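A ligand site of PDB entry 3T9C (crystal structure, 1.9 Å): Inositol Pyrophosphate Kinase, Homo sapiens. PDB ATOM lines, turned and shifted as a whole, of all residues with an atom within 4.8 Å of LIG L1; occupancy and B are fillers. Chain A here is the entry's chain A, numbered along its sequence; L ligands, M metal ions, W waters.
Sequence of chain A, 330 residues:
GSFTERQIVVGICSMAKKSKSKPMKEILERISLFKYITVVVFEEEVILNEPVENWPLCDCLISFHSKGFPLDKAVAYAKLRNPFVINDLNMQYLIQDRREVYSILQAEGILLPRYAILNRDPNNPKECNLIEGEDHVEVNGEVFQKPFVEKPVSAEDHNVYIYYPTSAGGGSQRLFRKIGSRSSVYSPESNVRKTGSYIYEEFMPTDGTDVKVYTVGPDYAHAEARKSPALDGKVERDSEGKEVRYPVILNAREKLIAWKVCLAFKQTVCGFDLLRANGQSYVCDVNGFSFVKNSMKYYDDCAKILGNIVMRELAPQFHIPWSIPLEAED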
ATOM      1  N   LYS A  17     -26.544 -11.889 -20.658  1.00  0.00           N
ATOM      2  CA  LYS A  17     -27.215 -12.498 -19.484  1.00  0.00           C
ATOM      3  C   LYS A  17     -26.223 -13.307 -18.631  1.00  0.00           C
ATOM      4  O   LYS A  17     -26.345 -13.382 -17.406  1.00  0.00           O
ATOM      5  CB  LYS A  17     -28.338 -13.412 -19.991  1.00  0.00           C
ATOM      6  CG  LYS A  17     -29.253 -13.986 -18.943  1.00  0.00           C
ATOM      7  CD  LYS A  17     -30.283 -14.902 -19.606  1.00  0.00           C
ATOM      8  CE  LYS A  17     -30.956 -15.809 -18.605  1.00  0.00           C
ATOM      9  NZ  LYS A  17     -32.234 -16.370 -19.136  1.00  0.00           N
ATOM     10  N   LYS A  18     -25.236 -13.891 -19.302  1.00  0.00           N
ATOM     11  CA  LYS A  18     -24.227 -14.677 -18.613  1.00  0.00           C
ATOM     12  C   LYS A  18     -23.014 -13.807 -18.248  1.00  0.00           C
ATOM     13  O   LYS A  18     -22.521 -13.886 -17.124  1.00  0.00           O
ATOM     14  CB  LYS A  18     -23.798 -15.868 -19.476  1.00  0.00           C
ATOM     15  CG  LYS A  18     -24.976 -16.728 -19.997  1.00  0.00           C
ATOM     16  CD  LYS A  18     -25.814 -17.346 -18.852  1.00  0.00           C
ATOM     17  CE  LYS A  18     -26.900 -18.262 -19.411  1.00  0.00           C
ATOM     18  NZ  LYS A  18     -27.831 -18.792 -18.367  1.00  0.00           N
ATOM     19  N   SER A  66     -25.181 -20.512 -24.667  1.00  0.00           N
ATOM     20  CA  SER A  66     -26.469 -20.559 -23.992  1.00  0.00           C
ATOM     21  C   SER A  66     -27.502 -20.091 -25.017  1.00  0.00           C
ATOM     22  O   SER A  66     -27.137 -19.799 -26.171  1.00  0.00           O
ATOM     23  CB  SER A  66     -26.486 -19.688 -22.729  1.00  0.00           C
ATOM     24  OG  SER A  66     -26.283 -18.314 -23.033  1.00  0.00           O
ATOM     25  N   LYS A  67     -28.765 -20.015 -24.625  1.00  0.00           N
ATOM     26  CA  LYS A  67     -29.832 -19.682 -25.559  1.00  0.00           C
ATOM     27  C   LYS A  67     -29.529 -18.414 -26.360  1.00  0.00           C
ATOM     28  O   LYS A  67     -29.272 -17.361 -25.781  1.00  0.00           O
ATOM     29  CB  LYS A  67     -31.175 -19.526 -24.811  1.00  0.00           C
ATOM     30  CG  LYS A  67     -32.350 -19.141 -25.732  1.00  0.00           C
ATOM     31  CD  LYS A  67     -33.684 -19.156 -24.981  1.00  0.00           C
ATOM     32  CE  LYS A  67     -34.798 -18.550 -25.823  1.00  0.00           C
ATOM     33  NZ  LYS A  67     -36.054 -18.352 -25.016  1.00  0.00           N
ATOM     34  N   HIS A 158     -36.223 -28.134 -21.176  1.00  0.00           N
ATOM     35  CA  HIS A 158     -36.303 -28.605 -19.779  1.00  0.00           C
ATOM     36  C   HIS A 158     -37.657 -29.224 -19.391  1.00  0.00           C
ATOM     37  O   HIS A 158     -37.914 -29.495 -18.208  1.00  0.00           O
ATOM     38  CB  HIS A 158     -35.905 -27.458 -18.852  1.00  0.00           C
ATOM     39  CG  HIS A 158     -34.541 -26.911 -19.172  1.00  0.00           C
ATOM     40  ND1 HIS A 158     -33.401 -27.659 -19.035  1.00  0.00           N
ATOM     41  CD2 HIS A 158     -34.159 -25.720 -19.704  1.00  0.00           C
ATOM     42  CE1 HIS A 158     -32.359 -26.949 -19.456  1.00  0.00           C
ATOM     43  NE2 HIS A 158     -32.793 -25.775 -19.859  1.00  0.00           N
ATOM     44  N   ARG A 177     -38.239 -25.186 -16.572  1.00  0.00           N
ATOM     45  CA  ARG A 177     -37.443 -24.100 -16.030  1.00  0.00           C
ATOM     46  C   ARG A 177     -38.283 -23.355 -15.004  1.00  0.00           C
ATOM     47  O   ARG A 177     -39.429 -23.006 -15.271  1.00  0.00           O
ATOM     48  CB  ARG A 177     -37.025 -23.109 -17.127  1.00  0.00           C
ATOM     49  CG  ARG A 177     -35.598 -23.244 -17.596  1.00  0.00           C
ATOM     50  CD  ARG A 177     -34.552 -22.718 -16.575  1.00  0.00           C
ATOM     51  NE  ARG A 177     -33.225 -23.144 -17.015  1.00  0.00           N
ATOM     52  CZ  ARG A 177     -32.691 -24.339 -16.732  1.00  0.00           C
ATOM     53  NH1 ARG A 177     -33.336 -25.208 -15.963  1.00  0.00           N
ATOM     54  NH2 ARG A 177     -31.494 -24.649 -17.199  1.00  0.00           N
ATOM     55  N   LYS A 178     -37.697 -23.151 -13.836  1.00  0.00           N
ATOM     56  CA  LYS A 178     -38.365 -22.511 -12.719  1.00  0.00           C
ATOM     57  C   LYS A 178     -39.147 -21.256 -13.151  1.00  0.00           C
ATOM     58  O   LYS A 178     -38.629 -20.389 -13.877  1.00  0.00           O
ATOM     59  CB  LYS A 178     -37.348 -22.210 -11.624  1.00  0.00           C
ATOM     60  CG  LYS A 178     -37.867 -21.479 -10.433  1.00  0.00           C
ATOM     61  CD  LYS A 178     -36.756 -21.281  -9.407  1.00  0.00           C
ATOM     62  CE  LYS A 178     -35.879 -20.075  -9.746  1.00  0.00           C
ATOM     63  NZ  LYS A 178     -34.647 -20.082  -8.897  1.00  0.00           N
ATOM     64  N   LYS A 212     -25.776 -31.320  -7.286  1.00  0.00           N
ATOM     65  CA  LYS A 212     -25.247 -30.487  -8.376  1.00  0.00           C
ATOM     66  C   LYS A 212     -23.758 -30.330  -8.188  1.00  0.00           C
ATOM     67  O   LYS A 212     -23.311 -29.942  -7.105  1.00  0.00           O
ATOM     68  CB  LYS A 212     -25.914 -29.121  -8.345  1.00  0.00           C
ATOM     69  CG  LYS A 212     -27.449 -29.181  -8.244  1.00  0.00           C
ATOM     70  CD  LYS A 212     -28.097 -29.285  -9.593  1.00  0.00           C
ATOM     71  CE  LYS A 212     -28.012 -27.970 -10.393  1.00  0.00           C
ATOM     72  NZ  LYS A 212     -28.219 -28.270 -11.854  1.00  0.00           N
ATOM     73  N   TYR A 214     -19.976 -28.775  -9.738  1.00  0.00           N
ATOM     74  CA  TYR A 214     -19.429 -27.661 -10.508  1.00  0.00           C
ATOM     75  C   TYR A 214     -17.901 -27.779 -10.501  1.00  0.00           C
ATOM     76  O   TYR A 214     -17.278 -27.625  -9.438  1.00  0.00           O
ATOM     77  CB  TYR A 214     -19.811 -26.332  -9.855  1.00  0.00           C
ATOM     78  CG  TYR A 214     -21.297 -26.079  -9.734  1.00  0.00           C
ATOM     79  CD1 TYR A 214     -22.019 -26.582  -8.638  1.00  0.00           C
ATOM     80  CD2 TYR A 214     -21.980 -25.315 -10.676  1.00  0.00           C
ATOM     81  CE1 TYR A 214     -23.400 -26.340  -8.512  1.00  0.00           C
ATOM     82  CE2 TYR A 214     -23.351 -25.073 -10.561  1.00  0.00           C
ATOM     83  CZ  TYR A 214     -24.050 -25.571  -9.471  1.00  0.00           C
ATOM     84  OH  TYR A 214     -25.423 -25.337  -9.338  1.00  0.00           O
ATOM     85  N   ARG A 226     -29.942 -29.962  -3.783  1.00  0.00           N
ATOM     86  CA  ARG A 226     -31.206 -29.216  -3.854  1.00  0.00           C
ATOM     87  C   ARG A 226     -32.350 -30.228  -3.881  1.00  0.00           C
ATOM     88  O   ARG A 226     -32.168 -31.371  -4.318  1.00  0.00           O
ATOM     89  CB  ARG A 226     -31.276 -28.362  -5.119  1.00  0.00           C
ATOM     90  CG  ARG A 226     -29.980 -27.668  -5.513  1.00  0.00           C
ATOM     91  CD  ARG A 226     -30.122 -26.166  -5.518  1.00  0.00           C
ATOM     92  NE  ARG A 226     -30.859 -25.711  -6.687  1.00  0.00           N
ATOM     93  CZ  ARG A 226     -30.304 -25.294  -7.825  1.00  0.00           C
ATOM     94  NH1 ARG A 226     -31.070 -24.895  -8.823  1.00  0.00           N
ATOM     95  NH2 ARG A 226     -28.986 -25.261  -7.945  1.00  0.00           N
ATOM     96  N   GLU A 243     -32.870 -20.062  -3.404  1.00  0.00           N
ATOM     97  CA  GLU A 243     -33.233 -21.480  -3.264  1.00  0.00           C
ATOM     98  C   GLU A 243     -32.373 -22.123  -2.188  1.00  0.00           C
ATOM     99  O   GLU A 243     -31.169 -21.871  -2.115  1.00  0.00           O
ATOM    100  CB  GLU A 243     -33.112 -22.236  -4.589  1.00  0.00           C
ATOM    101  CG  GLU A 243     -33.727 -23.647  -4.534  1.00  0.00           C
ATOM    102  CD  GLU A 243     -33.630 -24.412  -5.843  1.00  0.00           C
ATOM    103  OE1 GLU A 243     -32.992 -23.907  -6.792  1.00  0.00           O
ATOM    104  OE2 GLU A 243     -34.191 -25.520  -5.925  1.00  0.00           O
ATOM    105  N   ASN A 287     -24.349 -30.134 -18.087  1.00  0.00           N
ATOM    106  CA  ASN A 287     -24.736 -28.838 -18.641  1.00  0.00           C
ATOM    107  C   ASN A 287     -23.611 -28.006 -19.296  1.00  0.00           C
ATOM    108  O   ASN A 287     -23.903 -27.080 -20.057  1.00  0.00           O
ATOM    109  CB  ASN A 287     -25.467 -27.989 -17.582  1.00  0.00           C
ATOM    110  CG  ASN A 287     -26.702 -28.690 -17.055  1.00  0.00           C
ATOM    111  OD1 ASN A 287     -26.950 -28.726 -15.845  1.00  0.00           O
ATOM    112  ND2 ASN A 287     -27.483 -29.250 -17.969  1.00  0.00           N
ATOM    113  N   PHE A 289     -20.669 -25.134 -19.145  1.00  0.00           N
ATOM    114  CA  PHE A 289     -20.282 -23.961 -18.361  1.00  0.00           C
ATOM    115  C   PHE A 289     -21.335 -23.504 -17.358  1.00  0.00           C
ATOM    116  O   PHE A 289     -22.468 -23.214 -17.715  1.00  0.00           O
ATOM    117  CB  PHE A 289     -19.928 -22.782 -19.294  1.00  0.00           C
ATOM    118  CG  PHE A 289     -19.090 -21.753 -18.620  1.00  0.00           C
ATOM    119  CD1 PHE A 289     -19.667 -20.830 -17.734  1.00  0.00           C
ATOM    120  CD2 PHE A 289     -17.711 -21.703 -18.859  1.00  0.00           C
ATOM    121  CE1 PHE A 289     -18.881 -19.873 -17.085  1.00  0.00           C
ATOM    122  CE2 PHE A 289     -16.909 -20.758 -18.225  1.00  0.00           C
ATOM    123  CZ  PHE A 289     -17.496 -19.835 -17.329  1.00  0.00           C
ATOM    124  N   SER A 290     -20.948 -23.472 -16.096  1.00  0.00           N
ATOM    125  CA  SER A 290     -21.860 -23.110 -15.024  1.00  0.00           C
ATOM    126  C   SER A 290     -21.039 -22.763 -13.794  1.00  0.00           C
ATOM    127  O   SER A 290     -20.110 -23.489 -13.437  1.00  0.00           O
ATOM    128  CB  SER A 290     -22.836 -24.260 -14.712  1.00  0.00           C
ATOM    129  OG  SER A 290     -23.765 -23.814 -13.726  1.00  0.00           O
ATOM    130  N   LYS A 293     -23.436 -20.263  -7.494  1.00  0.00           N
ATOM    131  CA  LYS A 293     -24.035 -18.982  -7.143  1.00  0.00           C
ATOM    132  C   LYS A 293     -23.978 -18.802  -5.616  1.00  0.00           C
ATOM    133  O   LYS A 293     -24.105 -19.772  -4.879  1.00  0.00           O
ATOM    134  CB  LYS A 293     -25.476 -18.921  -7.660  1.00  0.00           C
ATOM    135  CG  LYS A 293     -25.622 -18.779  -9.186  1.00  0.00           C
ATOM    136  CD  LYS A 293     -25.529 -20.115  -9.911  1.00  0.00           C
ATOM    137  CE  LYS A 293     -25.774 -20.009 -11.419  1.00  0.00           C
ATOM    138  NZ  LYS A 293     -25.359 -21.276 -12.107  1.00  0.00           N
HETATM  139  C1  LIG L   1     -29.248 -22.723 -14.457  1.00  0.00           C
HETATM  140  C2  LIG L   1     -28.849 -21.891 -15.679  1.00  0.00           C
HETATM  141  C3  LIG L   1     -30.128 -21.247 -16.223  1.00  0.00           C
HETATM  142  C4  LIG L   1     -30.822 -20.347 -15.205  1.00  0.00           C
HETATM  143  C5  LIG L   1     -31.048 -21.043 -13.853  1.00  0.00           C
HETATM  144  C6  LIG L   1     -29.825 -21.817 -13.360  1.00  0.00           C
HETATM  145  O1  LIG L   1     -28.111 -23.437 -13.989  1.00  0.00           O
HETATM  146  P1  LIG L   1     -27.832 -24.933 -14.571  1.00  0.00           P
HETATM  147  O2  LIG L   1     -26.268 -25.079 -14.135  1.00  0.00           O
HETATM  148  O3  LIG L   1     -28.071 -25.158 -16.013  1.00  0.00           O
HETATM  149  O4  LIG L   1     -28.761 -25.949 -13.683  1.00  0.00           O
HETATM  150  O5  LIG L   1     -27.937 -20.891 -15.263  1.00  0.00           O
HETATM  151  P2  LIG L   1     -26.403 -20.976 -15.733  1.00  0.00           P
HETATM  152  O6  LIG L   1     -25.778 -19.608 -15.204  1.00  0.00           O
HETATM  153  O7  LIG L   1     -25.695 -22.176 -15.274  1.00  0.00           O
HETATM  154  O8  LIG L   1     -26.441 -20.788 -17.351  1.00  0.00           O
HETATM  155  O9  LIG L   1     -29.895 -20.533 -17.446  1.00  0.00           O
HETATM  156  P3  LIG L   1     -30.441 -21.228 -18.792  1.00  0.00           P
HETATM  157  O10 LIG L   1     -32.040 -21.034 -18.717  1.00  0.00           O
HETATM  158  O11 LIG L   1     -30.053 -22.669 -18.837  1.00  0.00           O
HETATM  159  O12 LIG L   1     -29.858 -20.280 -20.024  1.00  0.00           O
HETATM  160  O13 LIG L   1     -32.093 -20.071 -15.733  1.00  0.00           O
HETATM  161  P4  LIG L   1     -32.508 -18.590 -16.198  1.00  0.00           P
HETATM  162  O14 LIG L   1     -32.704 -18.725 -17.794  1.00  0.00           O
HETATM  163  O15 LIG L   1     -31.570 -17.524 -15.794  1.00  0.00           O
HETATM  164  O16 LIG L   1     -34.002 -18.492 -15.566  1.00  0.00           O
HETATM  165  O17 LIG L   1     -31.468 -20.062 -12.906  1.00  0.00           O
HETATM  166  P5  LIG L   1     -33.041 -20.067 -12.358  1.00  0.00           P
HETATM  167  O18 LIG L   1     -33.968 -20.991 -13.049  1.00  0.00           O
HETATM  168  O19 LIG L   1     -33.485 -18.521 -12.436  1.00  0.00           O
HETATM  169  O20 LIG L   1     -32.921 -20.387 -10.813  1.00  0.00           O
HETATM  170  O21 LIG L   1     -30.214 -22.651 -12.269  1.00  0.00           O
HETATM  171  P6  LIG L   1     -29.875 -22.156 -10.788  1.00  0.00           P
HETATM  172  O22 LIG L   1     -31.168 -22.580  -9.938  1.00  0.00           O
HETATM  173  O23 LIG L   1     -29.561 -20.700 -10.663  1.00  0.00           O
HETATM  174  O24 LIG L   1     -28.653 -23.081 -10.250  1.00  0.00           O
HETATM  175  P1  LG2 L   2     -31.019 -28.629 -15.845  1.00  0.00           P
HETATM  176  O1  LG2 L   2     -30.066 -29.136 -14.690  1.00  0.00           O
HETATM  177  O2  LG2 L   2     -31.608 -27.303 -15.474  1.00  0.00           O
HETATM  178  O3  LG2 L   2     -30.158 -28.509 -17.215  1.00  0.00           O
HETATM  179  P2  LG2 L   2     -32.500 -30.656 -17.338  1.00  0.00           P
HETATM  180  O4  LG2 L   2     -33.685 -30.241 -18.137  1.00  0.00           O
HETATM  181  O5  LG2 L   2     -31.240 -30.886 -18.081  1.00  0.00           O
HETATM  182  N1  LG2 L   2     -32.252 -29.763 -15.987  1.00  0.00           N
HETATM  183  P3  LG2 L   2     -32.281 -33.225 -15.897  1.00  0.00           P
HETATM  184  O6  LG2 L   2     -31.825 -34.354 -16.740  1.00  0.00           O
HETATM  185  O7  LG2 L   2     -31.332 -32.563 -15.000  1.00  0.00           O
HETATM  186  O8  LG2 L   2     -33.054 -32.075 -16.767  1.00  0.00           O
HETATM  187  O9  LG2 L   2     -33.558 -33.690 -15.052  1.00  0.00           O
HETATM  188  C1  LG2 L   2     -34.174 -32.739 -14.113  1.00  0.00           C
HETATM  189  C2  LG2 L   2     -34.455 -33.387 -12.735  1.00  0.00           C
HETATM  190  O10 LG2 L   2     -35.212 -34.560 -12.928  1.00  0.00           O
HETATM  191  C3  LG2 L   2     -33.155 -33.903 -12.155  1.00  0.00           C
HETATM  192  O11 LG2 L   2     -32.503 -32.854 -11.478  1.00  0.00           O
HETATM  193  C4  LG2 L   2     -33.663 -34.962 -11.183  1.00  0.00           C
HETATM  194  O12 LG2 L   2     -34.222 -34.359  -9.986  1.00  0.00           O
HETATM  195  C5  LG2 L   2     -34.809 -35.567 -11.996  1.00  0.00           C
HETATM  196  N2  LG2 L   2     -34.324 -36.749 -12.751  1.00  0.00           N
HETATM  197  C6  LG2 L   2     -33.683 -36.651 -14.074  1.00  0.00           C
HETATM  198  N3  LG2 L   2     -33.495 -38.038 -14.452  1.00  0.00           N
HETATM  199  C7  LG2 L   2     -33.834 -38.789 -13.408  1.00  0.00           C
HETATM  200  C8  LG2 L   2     -33.776 -40.161 -13.222  1.00  0.00           C
HETATM  201  N4  LG2 L   2     -33.309 -40.931 -14.205  1.00  0.00           N
HETATM  202  N5  LG2 L   2     -34.180 -40.692 -12.056  1.00  0.00           N
HETATM  203  C9  LG2 L   2     -34.634 -39.916 -11.070  1.00  0.00           C
HETATM  204  N6  LG2 L   2     -34.726 -38.586 -11.211  1.00  0.00           N
HETATM  205  C10 LG2 L   2     -34.335 -38.007 -12.369  1.00  0.00           C
HETATM  206 MG    MG M   1     -26.246 -23.963 -20.211  1.00  0.00          MG
HETATM  207  O   HOH W   1     -27.512 -22.789 -18.949  1.00  0.00           O
HETATM  208  O   HOH W   2     -30.336 -17.982 -21.233  1.00  0.00           O
HETATM  209  O   HOH W   3     -23.235 -17.265 -15.679  1.00  0.00           O
HETATM  210  O   HOH W   4     -33.747 -22.196 -20.401  1.00  0.00           O
HETATM  211  O   HOH W   5     -29.450 -21.421 -22.179  1.00  0.00           O
HETATM  212  O   HOH W   6     -23.166 -19.875 -14.543  1.00  0.00           O
HETATM  213  O   HOH W   7     -31.393 -17.221 -13.131  1.00  0.00           O
HETATM  214  O   HOH W   8     -28.967 -17.003 -16.640  1.00  0.00           O
HETATM  215  O   HOH W   9     -26.481 -23.818 -11.232  1.00  0.00           O
HETATM  216  O   HOH W  10     -35.991 -19.930 -14.145  1.00  0.00           O
HETATM  217  O   HOH W  11     -25.107 -27.229 -13.840  1.00  0.00           O
HETATM  218  O   HOH W  12     -28.855 -18.210 -11.500  1.00  0.00           O
HETATM  219  O   HOH W  13     -30.894 -24.214 -20.752  1.00  0.00           O
HETATM  220  O   HOH W  14     -24.090 -21.005 -18.517  1.00  0.00           O
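The side-chain amino group of Lys 293 is in salt-bridge range of an oxygen (O7) of LIG L1 (3.3 Å).
An oxygen (O8) of LIG L1 is in salt-bridge range of the side-chain amino group of Lys 18 (2.6 Å).
OG of Ser 290 is in hydrogen-bond range of O2 of LIG L1 (2.8 Å).
The guanidinium group (NH2) of Arg 177 is in salt-bridge range of an oxygen (O11) of LIG L1, at 2.9 Å.
NH1 of Arg 177 is in salt-bridge range of O2 of LG2 L2 (2.8 Å).
The guanidinium group (NH1) of Arg 226 is in salt-bridge range of an oxygen (O22) of LIG L1 (2.6 Å).
A ring nitrogen (ND1) of His 158 lies within hydrogen-bond range of an oxygen (O4) of LG2 L2.
NZ of Lys 212 lies close to O1 of LG2 L2 (3.5 Å).
NZ of Lys 212 is in salt-bridge range of O4 of LIG L1, 3.0 Å away.
NZ of Lys 17 is in salt-bridge range of O14 of LIG L1, at 2.8 Å.
NZ of Lys 178 is in salt-bridge range of O20 of LIG L1 (2.6 Å).
NZ of Lys 293 is in hydrogen-bond range of OG of Ser 290 (3.4 Å).
NE of Arg 226 is in salt-bridge range of OE1 of Glu 243 (2.8 Å).
The guanidinium group (NH2) of Arg 177 is in hydrogen-bond range of a ring nitrogen (NE2) of His 158.
Residues that only touch LIG L1: Glu 243 (3.9 Å) and Asn 287 (3.7 Å).
Water W11 lies within hydrogen-bond range of O2 of LIG L1 (2.5 Å) and OD1 of Asn 287 (3.1 Å).
Water W5 lies within hydrogen-bond range of an oxygen (O12) of LIG L1 (2.5 Å) and the backbone NH of Lys 67 (2.9 Å).
Water W9 lies within hydrogen-bond range of O24 of LIG L1 (2.5 Å), OH of Tyr 214 (2.6 Å) and NZ of Lys 293 (2.9 Å).
Water W13 lies within hydrogen-bond range of O11 of LIG L1 and NE2 of His 158.
Water W14 bridges O8 of LIG L1 and O of Phe 289.
Water W2 lies within hydrogen-bond range of O12 of LIG L1 (2.6 Å) and NZ of Lys 17 (3.3 Å).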
